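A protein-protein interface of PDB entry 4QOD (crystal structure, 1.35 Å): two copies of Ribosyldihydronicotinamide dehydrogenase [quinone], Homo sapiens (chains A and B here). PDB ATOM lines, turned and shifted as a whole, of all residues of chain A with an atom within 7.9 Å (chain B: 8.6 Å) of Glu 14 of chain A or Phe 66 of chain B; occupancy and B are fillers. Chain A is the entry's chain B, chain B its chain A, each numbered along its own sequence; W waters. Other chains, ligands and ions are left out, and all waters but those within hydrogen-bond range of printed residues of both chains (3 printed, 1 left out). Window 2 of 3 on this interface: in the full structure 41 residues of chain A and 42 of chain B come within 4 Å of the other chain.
No position is printed for both chains.
The side-chain carboxylate (OE1) of Glu 14 of chain A lies within hydrogen-bond range of the backbone NH (N) of Phe 66 of chain B (2.9 Å).
NE2 of Gln 13 of chain A is in hydrogen-bond range of O of Ala 51 of chain B (2.9 Å).
OG of Ser 17 of chain A is in hydrogen-bond range of O of Glu 14 of chain A (2.6 Å).
The backbone NH of Lys 16 of chain A is in hydrogen-bond range of the side-chain carboxylate of Glu 14 of chain A (2.9 Å).
NE2 of Gln 13 of chain A lies within hydrogen-bond range of OH of Tyr 43 of chain A, 3.3 Å away.
ND1 of His 12 of chain A lies within hydrogen-bond range of N of Glu 14 of chain A, at 3.0 Å.
N of Glu 64 of chain B sits at hydrogen-bond distance from OD1 of Asn 62 of chain B.
NE2 of Gln 13 of chain A sits at hydrogen-bond distance from OH of Tyr 105 of chain A.
Hydrophobic or aromatic side chains of chain B that line the printed part of chain A: Ala 51, Val 65, Phe 66 and Tyr 68.
Ala 11 of chain A touches none of the printed residues of chain B.
Of the printed residues of chain B, Gln 13 of chain A touches Ala 51, Phe 66 and Tyr 68.
Of chain B, only Glu 64, Val 65 and Phe 66 come within 4 Å of Glu 14 of chain A.
No residue of chain B comes within 4 Å of Pro 15 of chain A.
Of the printed residues of chain A, Ala 51 of chain B touches Gln 13 and Tyr 43.
Ser 61 of chain B touches none of the printed residues of chain A.
Of the printed residues of chain A, Phe 66 of chain B touches Gln 13 and Glu 14.
The nearest residue of chain B that does not touch Glu 14 of chain A is Pro 63 of chain B (5.6 Å).
The nearest printed residue of chain A that does not touch Glu 64 of chain B is Pro 15 of chain A (7.4 Å).
Water W3 lies within hydrogen-bond range of OE1 of Gln 13 of chain A (2.8 Å) and N of Tyr 68 of chain B (2.9 Å).
Water W1 lies within hydrogen-bond range of the side-chain hydroxyl (OH) of Tyr 43 of chain A (2.8 Å) and the backbone NH (N) of Ala 51 of chain B (3.4 Å).
Water W2 bridges the backbone carbonyl oxygen (O) of Gln 13 of chain A (3.3 Å) and the side-chain carboxylate (OD2) of Asp 53 of chain B (3.4 Å).
CD2 of Phe 66 of chain B touches CB of Gln 13 of chain A, at 3.999 Å.
Gln 13 of chain A touches Tyr 68 of chain B.
Glu 14 of chain A touches Glu 64 of chain B.
Glu 14 of chain A touches Val 65 of chain B.
O of Glu 64 of chain B touches NZ of Lys 16 of chain A (3.6 Å).
O of Ala 51 of chain B touches CE1 of Tyr 43 of chain A, at 3.3 Å.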
ATOM      1  N   TYR A  10      14.961  17.049 -28.005  1.00  0.00           N
ATOM      2  CA  TYR A  10      13.968  16.208 -27.374  1.00  0.00           C
ATOM      3  C   TYR A  10      12.721  16.084 -28.260  1.00  0.00           C
ATOM      4  O   TYR A  10      12.218  17.123 -28.701  1.00  0.00           O
ATOM      5  CB  TYR A  10      13.581  16.840 -26.026  1.00  0.00           C
ATOM      6  CG  TYR A  10      12.338  16.321 -25.328  1.00  0.00           C
ATOM      7  CD1 TYR A  10      12.234  15.053 -24.807  1.00  0.00           C
ATOM      8  CD2 TYR A  10      11.260  17.106 -25.222  1.00  0.00           C
ATOM      9  CE1 TYR A  10      11.139  14.537 -24.189  1.00  0.00           C
ATOM     10  CE2 TYR A  10      10.137  16.685 -24.583  1.00  0.00           C
ATOM     11  CZ  TYR A  10      10.047  15.405 -24.055  1.00  0.00           C
ATOM     12  OH  TYR A  10       8.954  14.917 -23.413  1.00  0.00           O
ATOM     13  N   ALA A  11      12.269  14.866 -28.518  1.00  0.00           N
ATOM     14  CA  ALA A  11      11.173  14.632 -29.451  1.00  0.00           C
ATOM     15  C   ALA A  11      10.117  13.709 -28.812  1.00  0.00           C
ATOM     16  O   ALA A  11       9.941  12.517 -29.210  1.00  0.00           O
ATOM     17  CB  ALA A  11      11.713  14.019 -30.761  1.00  0.00           C
ATOM     18  N   HIS A  12       9.285  14.268 -27.903  1.00  0.00           N
ATOM     19  CA  HIS A  12       8.122  13.569 -27.387  1.00  0.00           C
ATOM     20  C   HIS A  12       7.027  14.568 -27.100  1.00  0.00           C
ATOM     21  O   HIS A  12       7.274  15.702 -26.680  1.00  0.00           O
ATOM     22  CB  HIS A  12       8.420  12.743 -26.156  1.00  0.00           C
ATOM     23  CG  HIS A  12       7.435  11.657 -25.921  1.00  0.00           C
ATOM     24  ND1 HIS A  12       6.166  11.898 -25.478  1.00  0.00           N
ATOM     25  CD2 HIS A  12       7.499  10.335 -26.134  1.00  0.00           C
ATOM     26  CE1 HIS A  12       5.505  10.763 -25.367  1.00  0.00           C
ATOM     27  NE2 HIS A  12       6.302   9.803 -25.784  1.00  0.00           N
ATOM     28  N   GLN A  13       5.813  14.140 -27.457  1.00  0.00           N
ATOM     29  CA  GLN A  13       4.635  15.005 -27.335  1.00  0.00           C
ATOM     30  C   GLN A  13       4.148  15.263 -25.909  1.00  0.00           C
ATOM     31  O   GLN A  13       3.416  16.231 -25.705  1.00  0.00           O
ATOM     32  CB  GLN A  13       3.466  14.452 -28.136  1.00  0.00           C
ATOM     33  CG  GLN A  13       3.782  14.003 -29.564  1.00  0.00           C
ATOM     34  CD  GLN A  13       4.274  12.588 -29.684  1.00  0.00           C
ATOM     35  OE1 GLN A  13       4.710  11.942 -28.732  1.00  0.00           O
ATOM     36  NE2 GLN A  13       4.198  12.065 -30.914  1.00  0.00           N
ATOM     37  N   GLU A  14       4.506  14.383 -24.988  1.00  0.00           N
ATOM     38  CA  GLU A  14       3.955  14.416 -23.667  1.00  0.00           C
ATOM     39  C   GLU A  14       4.973  14.559 -22.533  1.00  0.00           C
ATOM     40  O   GLU A  14       5.831  13.700 -22.322  1.00  0.00           O
ATOM     41  CB  GLU A  14       3.221  13.095 -23.489  1.00  0.00           C
ATOM     42  CG  GLU A  14       2.593  12.820 -22.115  1.00  0.00           C
ATOM     43  CD  GLU A  14       1.704  13.934 -21.657  1.00  0.00           C
ATOM     44  OE1 GLU A  14       0.569  14.045 -22.190  1.00  0.00           O
ATOM     45  OE2 GLU A  14       2.079  14.655 -20.690  1.00  0.00           O
ATOM     46  N   PRO A  15       4.837  15.640 -21.781  1.00  0.00           N
ATOM     47  CA  PRO A  15       5.801  15.911 -20.719  1.00  0.00           C
ATOM     48  C   PRO A  15       5.787  14.882 -19.624  1.00  0.00           C
ATOM     49  O   PRO A  15       6.824  14.668 -18.983  1.00  0.00           O
ATOM     50  CB  PRO A  15       5.351  17.288 -20.186  1.00  0.00           C
ATOM     51  CG  PRO A  15       4.311  17.820 -21.003  1.00  0.00           C
ATOM     52  CD  PRO A  15       4.009  16.834 -22.074  1.00  0.00           C
ATOM     53  N   LYS A  16       4.627  14.244 -19.410  1.00  0.00           N
ATOM     54  CA  LYS A  16       4.509  13.184 -18.403  1.00  0.00           C
ATOM     55  C   LYS A  16       5.030  11.834 -18.824  1.00  0.00           C
ATOM     56  O   LYS A  16       4.983  10.871 -18.090  1.00  0.00           O
ATOM     57  CB  LYS A  16       3.073  13.068 -17.957  1.00  0.00           C
ATOM     58  CG  LYS A  16       2.574  14.316 -17.296  1.00  0.00           C
ATOM     59  CD  LYS A  16       1.178  14.058 -16.820  1.00  0.00           C
ATOM     60  CE  LYS A  16       0.555  15.313 -16.261  1.00  0.00           C
ATOM     61  NZ  LYS A  16      -0.887  15.017 -15.985  1.00  0.00           N
ATOM     62  N   SER A  17       5.520  11.744 -20.076  1.00  0.00           N
ATOM     63  CA  SER A  17       6.060  10.476 -20.572  1.00  0.00           C
ATOM     64  C   SER A  17       7.346  10.035 -19.957  1.00  0.00           C
ATOM     65  O   SER A  17       8.062  10.861 -19.335  1.00  0.00           O
ATOM     66  CB  SER A  17       6.185  10.575 -22.066  1.00  0.00           C
ATOM     67  OG  SER A  17       7.262  11.480 -22.447  1.00  0.00           O
ATOM     68  N   PHE A  18       7.731   8.797 -20.229  1.00  0.00           N
ATOM     69  CA  PHE A  18       9.046   8.278 -19.819  1.00  0.00           C
ATOM     70  C   PHE A  18      10.130   9.018 -20.537  1.00  0.00           C
ATOM     71  O   PHE A  18      11.167   9.352 -19.944  1.00  0.00           O
ATOM     72  CB  PHE A  18       9.117   6.783 -20.086  1.00  0.00           C
ATOM     73  CG  PHE A  18      10.347   6.129 -19.562  1.00  0.00           C
ATOM     74  CD1 PHE A  18      10.461   5.867 -18.199  1.00  0.00           C
ATOM     75  CD2 PHE A  18      11.355   5.746 -20.411  1.00  0.00           C
ATOM     76  CE1 PHE A  18      11.608   5.306 -17.707  1.00  0.00           C
ATOM     77  CE2 PHE A  18      12.494   5.155 -19.910  1.00  0.00           C
ATOM     78  CZ  PHE A  18      12.597   4.895 -18.570  1.00  0.00           C
ATOM     79  N   ASN A  19       9.952   9.339 -21.820  1.00  0.00           N
ATOM     80  CA  ASN A  19      10.911  10.172 -22.526  1.00  0.00           C
ATOM     81  C   ASN A  19      11.068  11.556 -21.812  1.00  0.00           C
ATOM     82  O   ASN A  19      12.162  12.056 -21.633  1.00  0.00           O
ATOM     83  CB  ASN A  19      10.487  10.406 -23.995  1.00  0.00           C
ATOM     84  CG  ASN A  19      11.067   9.362 -24.939  1.00  0.00           C
ATOM     85  OD1 ASN A  19      12.180   9.507 -25.469  1.00  0.00           O
ATOM     86  ND2 ASN A  19      10.316   8.242 -25.120  1.00  0.00           N
ATOM     87  N   GLY A  20       9.971  12.139 -21.440  1.00  0.00           N
ATOM     88  CA  GLY A  20       9.998  13.401 -20.652  1.00  0.00           C
ATOM     89  C   GLY A  20      10.796  13.224 -19.351  1.00  0.00           C
ATOM     90  O   GLY A  20      11.515  14.113 -18.977  1.00  0.00           O
ATOM     91  N   SER A  21      10.564  12.133 -18.642  1.00  0.00           N
ATOM     92  CA  SER A  21      11.316  11.862 -17.409  1.00  0.00           C
ATOM     93  C   SER A  21      12.812  11.802 -17.691  1.00  0.00           C
ATOM     94  O   SER A  21      13.587  12.302 -16.880  1.00  0.00           O
ATOM     95  CB  SER A  21      10.797  10.598 -16.756  1.00  0.00           C
ATOM     96  OG  SER A  21       9.480  10.821 -16.330  1.00  0.00           O
ATOM     97  N   LYS A  23      14.452  13.163 -20.148  1.00  0.00           N
ATOM     98  CA  LYS A  23      14.931  14.492 -20.496  1.00  0.00           C
ATOM     99  C   LYS A  23      15.069  15.334 -19.217  1.00  0.00           C
ATOM    100  O   LYS A  23      16.078  16.013 -19.030  1.00  0.00           O
ATOM    101  CB  LYS A  23      13.926  15.156 -21.461  1.00  0.00           C
ATOM    102  CG  LYS A  23      14.311  16.548 -21.861  1.00  0.00           C
ATOM    103  CD  LYS A  23      13.686  17.658 -21.043  1.00  0.00           C
ATOM    104  CE  LYS A  23      12.187  17.738 -21.373  1.00  0.00           C
ATOM    105  NZ  LYS A  23      11.493  18.734 -20.510  1.00  0.00           N
ATOM    106  N   ASN A  24      14.102  15.273 -18.335  1.00  0.00           N
ATOM    107  CA  ASN A  24      14.166  16.055 -17.132  1.00  0.00           C
ATOM    108  C   ASN A  24      15.279  15.622 -16.183  1.00  0.00           C
ATOM    109  O   ASN A  24      15.906  16.502 -15.555  1.00  0.00           O
ATOM    110  CB  ASN A  24      12.813  16.074 -16.421  1.00  0.00           C
ATOM    111  CG  ASN A  24      11.745  16.816 -17.180  1.00  0.00           C
ATOM    112  OD1 ASN A  24      12.057  17.724 -17.955  1.00  0.00           O
ATOM    113  ND2 ASN A  24      10.527  16.443 -17.006  1.00  0.00           N
ATOM    114  N   ASP A  41      12.807  21.459 -27.495  1.00  0.00           N
ATOM    115  CA  ASP A  41      11.635  20.613 -27.246  1.00  0.00           C
ATOM    116  C   ASP A  41      10.850  20.732 -28.591  1.00  0.00           C
ATOM    117  O   ASP A  41      10.050  21.648 -28.800  1.00  0.00           O
ATOM    118  CB  ASP A  41      10.837  21.158 -26.114  1.00  0.00           C
ATOM    119  CG  ASP A  41       9.611  20.302 -25.755  1.00  0.00           C
ATOM    120  OD1 ASP A  41       9.095  19.580 -26.637  1.00  0.00           O
ATOM    121  OD2 ASP A  41       9.082  20.515 -24.636  1.00  0.00           O
ATOM    122  N   TYR A  43       8.421  19.256 -30.393  1.00  0.00           N
ATOM    123  CA  TYR A  43       6.966  19.352 -30.517  1.00  0.00           C
ATOM    124  C   TYR A  43       6.425  20.640 -29.896  1.00  0.00           C
ATOM    125  O   TYR A  43       5.542  21.292 -30.489  1.00  0.00           O
ATOM    126  CB  TYR A  43       6.260  18.168 -29.917  1.00  0.00           C
ATOM    127  CG  TYR A  43       6.404  16.839 -30.648  1.00  0.00           C
ATOM    128  CD1 TYR A  43       5.706  16.599 -31.790  1.00  0.00           C
ATOM    129  CD2 TYR A  43       7.257  15.882 -30.205  1.00  0.00           C
ATOM    130  CE1 TYR A  43       5.829  15.413 -32.527  1.00  0.00           C
ATOM    131  CE2 TYR A  43       7.373  14.657 -30.858  1.00  0.00           C
ATOM    132  CZ  TYR A  43       6.625  14.386 -31.995  1.00  0.00           C
ATOM    133  OH  TYR A  43       6.785  13.221 -32.684  1.00  0.00           O
ATOM    134  N   TYR A 105      10.675   5.324 -33.679  1.00  0.00           N
ATOM    135  CA  TYR A 105       9.537   5.245 -34.612  1.00  0.00           C
ATOM    136  C   TYR A 105      10.062   4.561 -35.878  1.00  0.00           C
ATOM    137  O   TYR A 105      10.939   5.131 -36.524  1.00  0.00           O
ATOM    138  CB  TYR A 105       8.953   6.618 -34.977  1.00  0.00           C
ATOM    139  CG  TYR A 105       8.021   7.283 -33.993  1.00  0.00           C
ATOM    140  CD1 TYR A 105       7.920   6.906 -32.717  1.00  0.00           C
ATOM    141  CD2 TYR A 105       7.292   8.373 -34.392  1.00  0.00           C
ATOM    142  CE1 TYR A 105       7.094   7.562 -31.811  1.00  0.00           C
ATOM    143  CE2 TYR A 105       6.454   9.015 -33.507  1.00  0.00           C
ATOM    144  CZ  TYR A 105       6.360   8.595 -32.219  1.00  0.00           C
ATOM    145  OH  TYR A 105       5.537   9.284 -31.343  1.00  0.00           O
ATOM    146  N   ALA B  51       3.723  13.729 -35.785  1.00  0.00           N
ATOM    147  CA  ALA B  51       2.801  12.874 -35.057  1.00  0.00           C
ATOM    148  C   ALA B  51       2.303  13.627 -33.822  1.00  0.00           C
ATOM    149  O   ALA B  51       2.978  13.737 -32.880  1.00  0.00           O
ATOM    150  CB  ALA B  51       3.495  11.599 -34.653  1.00  0.00           C
ATOM    151  N   THR B  52       1.107  14.181 -33.933  1.00  0.00           N
ATOM    152  CA  THR B  52       0.548  14.999 -32.862  1.00  0.00           C
ATOM    153  C   THR B  52      -0.893  14.606 -32.520  1.00  0.00           C
ATOM    154  O   THR B  52      -1.528  13.894 -33.221  1.00  0.00           O
ATOM    155  CB  THR B  52       0.598  16.510 -33.157  1.00  0.00           C
ATOM    156  OG1 THR B  52      -0.486  16.866 -34.009  1.00  0.00           O
ATOM    157  CG2 THR B  52       1.926  16.925 -33.773  1.00  0.00           C
ATOM    158  N   ASP B  53      -1.362  15.186 -31.420  1.00  0.00           N
ATOM    159  CA  ASP B  53      -2.715  14.960 -30.961  1.00  0.00           C
ATOM    160  C   ASP B  53      -3.776  15.530 -31.889  1.00  0.00           C
ATOM    161  O   ASP B  53      -4.883  15.202 -31.747  1.00  0.00           O
ATOM    162  CB  ASP B  53      -2.895  15.467 -29.526  1.00  0.00           C
ATOM    163  CG  ASP B  53      -2.694  16.966 -29.377  1.00  0.00           C
ATOM    164  OD1 ASP B  53      -2.608  17.724 -30.292  1.00  0.00           O
ATOM    165  OD2 ASP B  53      -2.615  17.380 -28.241  1.00  0.00           O
ATOM    166  N   LYS B  54      -3.371  16.324 -32.861  1.00  0.00           N
ATOM    167  CA  LYS B  54      -4.265  16.812 -33.895  1.00  0.00           C
ATOM    168  C   LYS B  54      -4.693  15.696 -34.873  1.00  0.00           C
ATOM    169  O   LYS B  54      -5.606  15.868 -35.611  1.00  0.00           O
ATOM    170  CB  LYS B  54      -3.659  17.994 -34.661  1.00  0.00           C
ATOM    171  CG  LYS B  54      -3.370  19.297 -33.877  1.00  0.00           C
ATOM    172  CD  LYS B  54      -4.649  19.999 -33.431  1.00  0.00           C
ATOM    173  CE  LYS B  54      -4.589  20.715 -32.080  1.00  0.00           C
ATOM    174  NZ  LYS B  54      -4.986  19.889 -30.882  1.00  0.00           N
ATOM    175  N   ASP B  55      -4.025  14.554 -34.821  1.00  0.00           N
ATOM    176  CA  ASP B  55      -4.348  13.426 -35.690  1.00  0.00           C
ATOM    177  C   ASP B  55      -5.541  12.602 -35.278  1.00  0.00           C
ATOM    178  O   ASP B  55      -5.998  11.718 -35.966  1.00  0.00           O
ATOM    179  CB  ASP B  55      -3.106  12.500 -35.804  1.00  0.00           C
ATOM    180  CG  ASP B  55      -1.992  13.178 -36.549  1.00  0.00           C
ATOM    181  OD1 ASP B  55      -2.174  14.293 -37.161  1.00  0.00           O
ATOM    182  OD2 ASP B  55      -0.831  12.631 -36.580  1.00  0.00           O
ATOM    183  N   ILE B  56      -6.073  12.953 -34.102  1.00  0.00           N
ATOM    184  CA  ILE B  56      -7.238  12.265 -33.564  1.00  0.00           C
ATOM    185  C   ILE B  56      -8.331  13.346 -33.306  1.00  0.00           C
ATOM    186  O   ILE B  56      -8.069  14.354 -32.697  1.00  0.00           O
ATOM    187  CB  ILE B  56      -7.006  11.514 -32.226  1.00  0.00           C
ATOM    188  CG1 ILE B  56      -5.894  10.446 -32.406  1.00  0.00           C
ATOM    189  CG2 ILE B  56      -8.348  10.986 -31.703  1.00  0.00           C
ATOM    190  CD1 ILE B  56      -4.590  10.964 -31.869  1.00  0.00           C
ATOM    191  N   GLY B  58     -11.756  12.657 -32.210  1.00  0.00           N
ATOM    192  CA  GLY B  58     -12.571  12.636 -30.934  1.00  0.00           C
ATOM    193  C   GLY B  58     -12.012  12.687 -29.496  1.00  0.00           C
ATOM    194  O   GLY B  58     -10.885  13.075 -29.244  1.00  0.00           O
ATOM    195  N   LEU B  60     -10.221  11.418 -26.355  1.00  0.00           N
ATOM    196  CA  LEU B  60      -9.040  10.575 -26.243  1.00  0.00           C
ATOM    197  C   LEU B  60      -9.320   9.500 -25.227  1.00  0.00           C
ATOM    198  O   LEU B  60     -10.134   9.666 -24.273  1.00  0.00           O
ATOM    199  CB  LEU B  60      -7.846  11.388 -25.848  1.00  0.00           C
ATOM    200  CG  LEU B  60      -7.353  12.408 -26.892  1.00  0.00           C
ATOM    201  CD1 LEU B  60      -6.194  13.146 -26.325  1.00  0.00           C
ATOM    202  CD2 LEU B  60      -6.987  11.726 -28.216  1.00  0.00           C
ATOM    203  N   SER B  61      -8.666   8.374 -25.415  1.00  0.00           N
ATOM    204  CA  SER B  61      -8.733   7.299 -24.513  1.00  0.00           C
ATOM    205  C   SER B  61      -8.110   7.652 -23.120  1.00  0.00           C
ATOM    206  O   SER B  61      -8.657   7.330 -22.056  1.00  0.00           O
ATOM    207  CB  SER B  61      -8.036   6.108 -25.180  1.00  0.00           C
ATOM    208  OG  SER B  61      -7.985   5.047 -24.311  1.00  0.00           O
ATOM    209  N   ASN B  62      -6.992   8.350 -23.133  1.00  0.00           N
ATOM    210  CA  ASN B  62      -6.332   8.835 -21.940  1.00  0.00           C
ATOM    211  C   ASN B  62      -5.867  10.249 -22.128  1.00  0.00           C
ATOM    212  O   ASN B  62      -4.716  10.501 -22.464  1.00  0.00           O
ATOM    213  CB  ASN B  62      -5.136   7.934 -21.551  1.00  0.00           C
ATOM    214  CG  ASN B  62      -4.487   8.347 -20.220  1.00  0.00           C
ATOM    215  OD1 ASN B  62      -4.695   9.477 -19.676  1.00  0.00           O
ATOM    216  ND2 ASN B  62      -3.696   7.443 -19.677  1.00  0.00           N
ATOM    217  N   PRO B  63      -6.748  11.205 -21.869  1.00  0.00           N
ATOM    218  CA  PRO B  63      -6.370  12.582 -22.134  1.00  0.00           C
ATOM    219  C   PRO B  63      -5.398  13.132 -21.093  1.00  0.00           C
ATOM    220  O   PRO B  63      -4.907  14.230 -21.295  1.00  0.00           O
ATOM    221  CB  PRO B  63      -7.701  13.342 -22.100  1.00  0.00           C
ATOM    222  CG  PRO B  63      -8.608  12.497 -21.288  1.00  0.00           C
ATOM    223  CD  PRO B  63      -8.148  11.073 -21.425  1.00  0.00           C
ATOM    224  N   GLU B  64      -5.120  12.385 -20.021  1.00  0.00           N
ATOM    225  CA  GLU B  64      -4.158  12.873 -19.020  1.00  0.00           C
ATOM    226  C   GLU B  64      -2.685  12.684 -19.463  1.00  0.00           C
ATOM    227  O   GLU B  64      -1.829  13.483 -19.121  1.00  0.00           O
ATOM    228  CB  GLU B  64      -4.420  12.180 -17.635  1.00  0.00           C
ATOM    229  CG  GLU B  64      -5.866  12.219 -17.120  1.00  0.00           C
ATOM    230  CD  GLU B  64      -6.310  13.616 -16.728  1.00  0.00           C
ATOM    231  OE1 GLU B  64      -6.294  14.517 -17.612  1.00  0.00           O
ATOM    232  OE2 GLU B  64      -6.674  13.804 -15.523  1.00  0.00           O
ATOM    233  N   VAL B  65      -2.424  11.596 -20.174  1.00  0.00           N
ATOM    234  CA  VAL B  65      -1.089  11.192 -20.549  1.00  0.00           C
ATOM    235  C   VAL B  65      -1.216  10.697 -22.016  1.00  0.00           C
ATOM    236  O   VAL B  65      -1.717   9.577 -22.285  1.00  0.00           O
ATOM    237  CB  VAL B  65      -0.489  10.071 -19.710  1.00  0.00           C
ATOM    238  CG1 VAL B  65       0.953   9.832 -20.182  1.00  0.00           C
ATOM    239  CG2 VAL B  65      -0.522  10.461 -18.243  1.00  0.00           C
ATOM    240  N   PHE B  66      -0.802  11.619 -22.914  1.00  0.00           N
ATOM    241  CA  PHE B  66      -0.974  11.381 -24.351  1.00  0.00           C
ATOM    242  C   PHE B  66       0.077  10.358 -24.863  1.00  0.00           C
ATOM    243  O   PHE B  66       1.274  10.625 -24.728  1.00  0.00           O
ATOM    244  CB  PHE B  66      -0.844  12.666 -25.158  1.00  0.00           C
ATOM    245  CG  PHE B  66      -1.072  12.457 -26.642  1.00  0.00           C
ATOM    246  CD1 PHE B  66      -2.311  12.287 -27.167  1.00  0.00           C
ATOM    247  CD2 PHE B  66      -0.001  12.561 -27.505  1.00  0.00           C
ATOM    248  CE1 PHE B  66      -2.521  12.015 -28.519  1.00  0.00           C
ATOM    249  CE2 PHE B  66      -0.170  12.365 -28.848  1.00  0.00           C
ATOM    250  CZ  PHE B  66      -1.446  12.073 -29.353  1.00  0.00           C
ATOM    251  N   ASN B  67      -0.379   9.291 -25.507  1.00  0.00           N
ATOM    252  CA  ASN B  67       0.449   8.284 -26.143  1.00  0.00           C
ATOM    253  C   ASN B  67      -0.025   8.157 -27.573  1.00  0.00           C
ATOM    254  O   ASN B  67      -1.146   7.684 -27.818  1.00  0.00           O
ATOM    255  CB  ASN B  67       0.269   6.988 -25.392  1.00  0.00           C
ATOM    256  CG  ASN B  67       1.143   5.842 -25.898  1.00  0.00           C
ATOM    257  OD1 ASN B  67       1.175   5.535 -27.104  1.00  0.00           O
ATOM    258  ND2 ASN B  67       1.804   5.132 -24.940  1.00  0.00           N
ATOM    259  N   TYR B  68       0.821   8.633 -28.470  1.00  0.00           N
ATOM    260  CA  TYR B  68       0.430   8.668 -29.878  1.00  0.00           C
ATOM    261  C   TYR B  68      -0.010   7.321 -30.446  1.00  0.00           C
ATOM    262  O   TYR B  68      -1.060   7.264 -31.177  1.00  0.00           O
ATOM    263  CB  TYR B  68       1.519   9.316 -30.708  1.00  0.00           C
ATOM    264  CG  TYR B  68       1.141   9.546 -32.179  1.00  0.00           C
ATOM    265  CD1 TYR B  68       0.406  10.698 -32.520  1.00  0.00           C
ATOM    266  CD2 TYR B  68       1.415   8.634 -33.152  1.00  0.00           C
ATOM    267  CE1 TYR B  68       0.049  10.935 -33.853  1.00  0.00           C
ATOM    268  CE2 TYR B  68       1.059   8.820 -34.442  1.00  0.00           C
ATOM    269  CZ  TYR B  68       0.329   9.969 -34.816  1.00  0.00           C
ATOM    270  OH  TYR B  68      -0.122  10.178 -36.094  1.00  0.00           O
ATOM    271  N   GLY B  69       0.787   6.270 -30.183  1.00  0.00           N
ATOM    272  CA  GLY B  69       0.437   4.983 -30.709  1.00  0.00           C
ATOM    273  C   GLY B  69      -0.912   4.444 -30.199  1.00  0.00           C
ATOM    274  O   GLY B  69      -1.696   3.920 -30.959  1.00  0.00           O
ATOM    275  N   VAL B  70      -1.138   4.629 -28.942  1.00  0.00           N
ATOM    276  CA  VAL B  70      -2.363   4.104 -28.339  1.00  0.00           C
ATOM    277  C   VAL B  70      -3.588   4.869 -28.879  1.00  0.00           C
ATOM    278  O   VAL B  70      -4.586   4.263 -29.257  1.00  0.00           O
ATOM    279  CB  VAL B  70      -2.364   4.245 -26.799  1.00  0.00           C
ATOM    280  CG1 VAL B  70      -3.780   4.040 -26.185  1.00  0.00           C
ATOM    281  CG2 VAL B  70      -1.355   3.279 -26.238  1.00  0.00           C
ATOM    282  N   GLU B  71      -3.462   6.193 -28.935  1.00  0.00           N
ATOM    283  CA  GLU B  71      -4.550   7.021 -29.354  1.00  0.00           C
ATOM    284  C   GLU B  71      -4.839   6.911 -30.849  1.00  0.00           C
ATOM    285  O   GLU B  71      -6.026   6.907 -31.239  1.00  0.00           O
ATOM    286  CB  GLU B  71      -4.330   8.434 -29.006  1.00  0.00           C
ATOM    287  CG  GLU B  71      -4.254   8.817 -27.521  1.00  0.00           C
ATOM    288  CD  GLU B  71      -5.493   8.553 -26.694  1.00  0.00           C
ATOM    289  OE1 GLU B  71      -6.557   8.349 -27.286  1.00  0.00           O
ATOM    290  OE2 GLU B  71      -5.422   8.572 -25.447  1.00  0.00           O
ATOM    291  N   THR B  72      -3.822   6.725 -31.679  1.00  0.00           N
ATOM    292  CA  THR B  72      -4.115   6.516 -33.114  1.00  0.00           C
ATOM    293  C   THR B  72      -4.701   5.134 -33.366  1.00  0.00           C
ATOM    294  O   THR B  72      -5.485   4.969 -34.299  1.00  0.00           O
ATOM    295  CB  THR B  72      -2.895   6.868 -33.994  1.00  0.00           C
ATOM    296  OG1 THR B  72      -1.778   6.050 -33.602  1.00  0.00           O
ATOM    297  CG2 THR B  72      -2.564   8.318 -33.919  1.00  0.00           C
HETATM  298  O   HOH W   1       7.091  13.521 -35.488  1.00  0.00           O
HETATM  299  O   HOH W   2       0.381  16.414 -26.960  1.00  0.00           O
HETATM  300  O   HOH W   3       3.313   9.769 -27.623  1.00  0.00           O
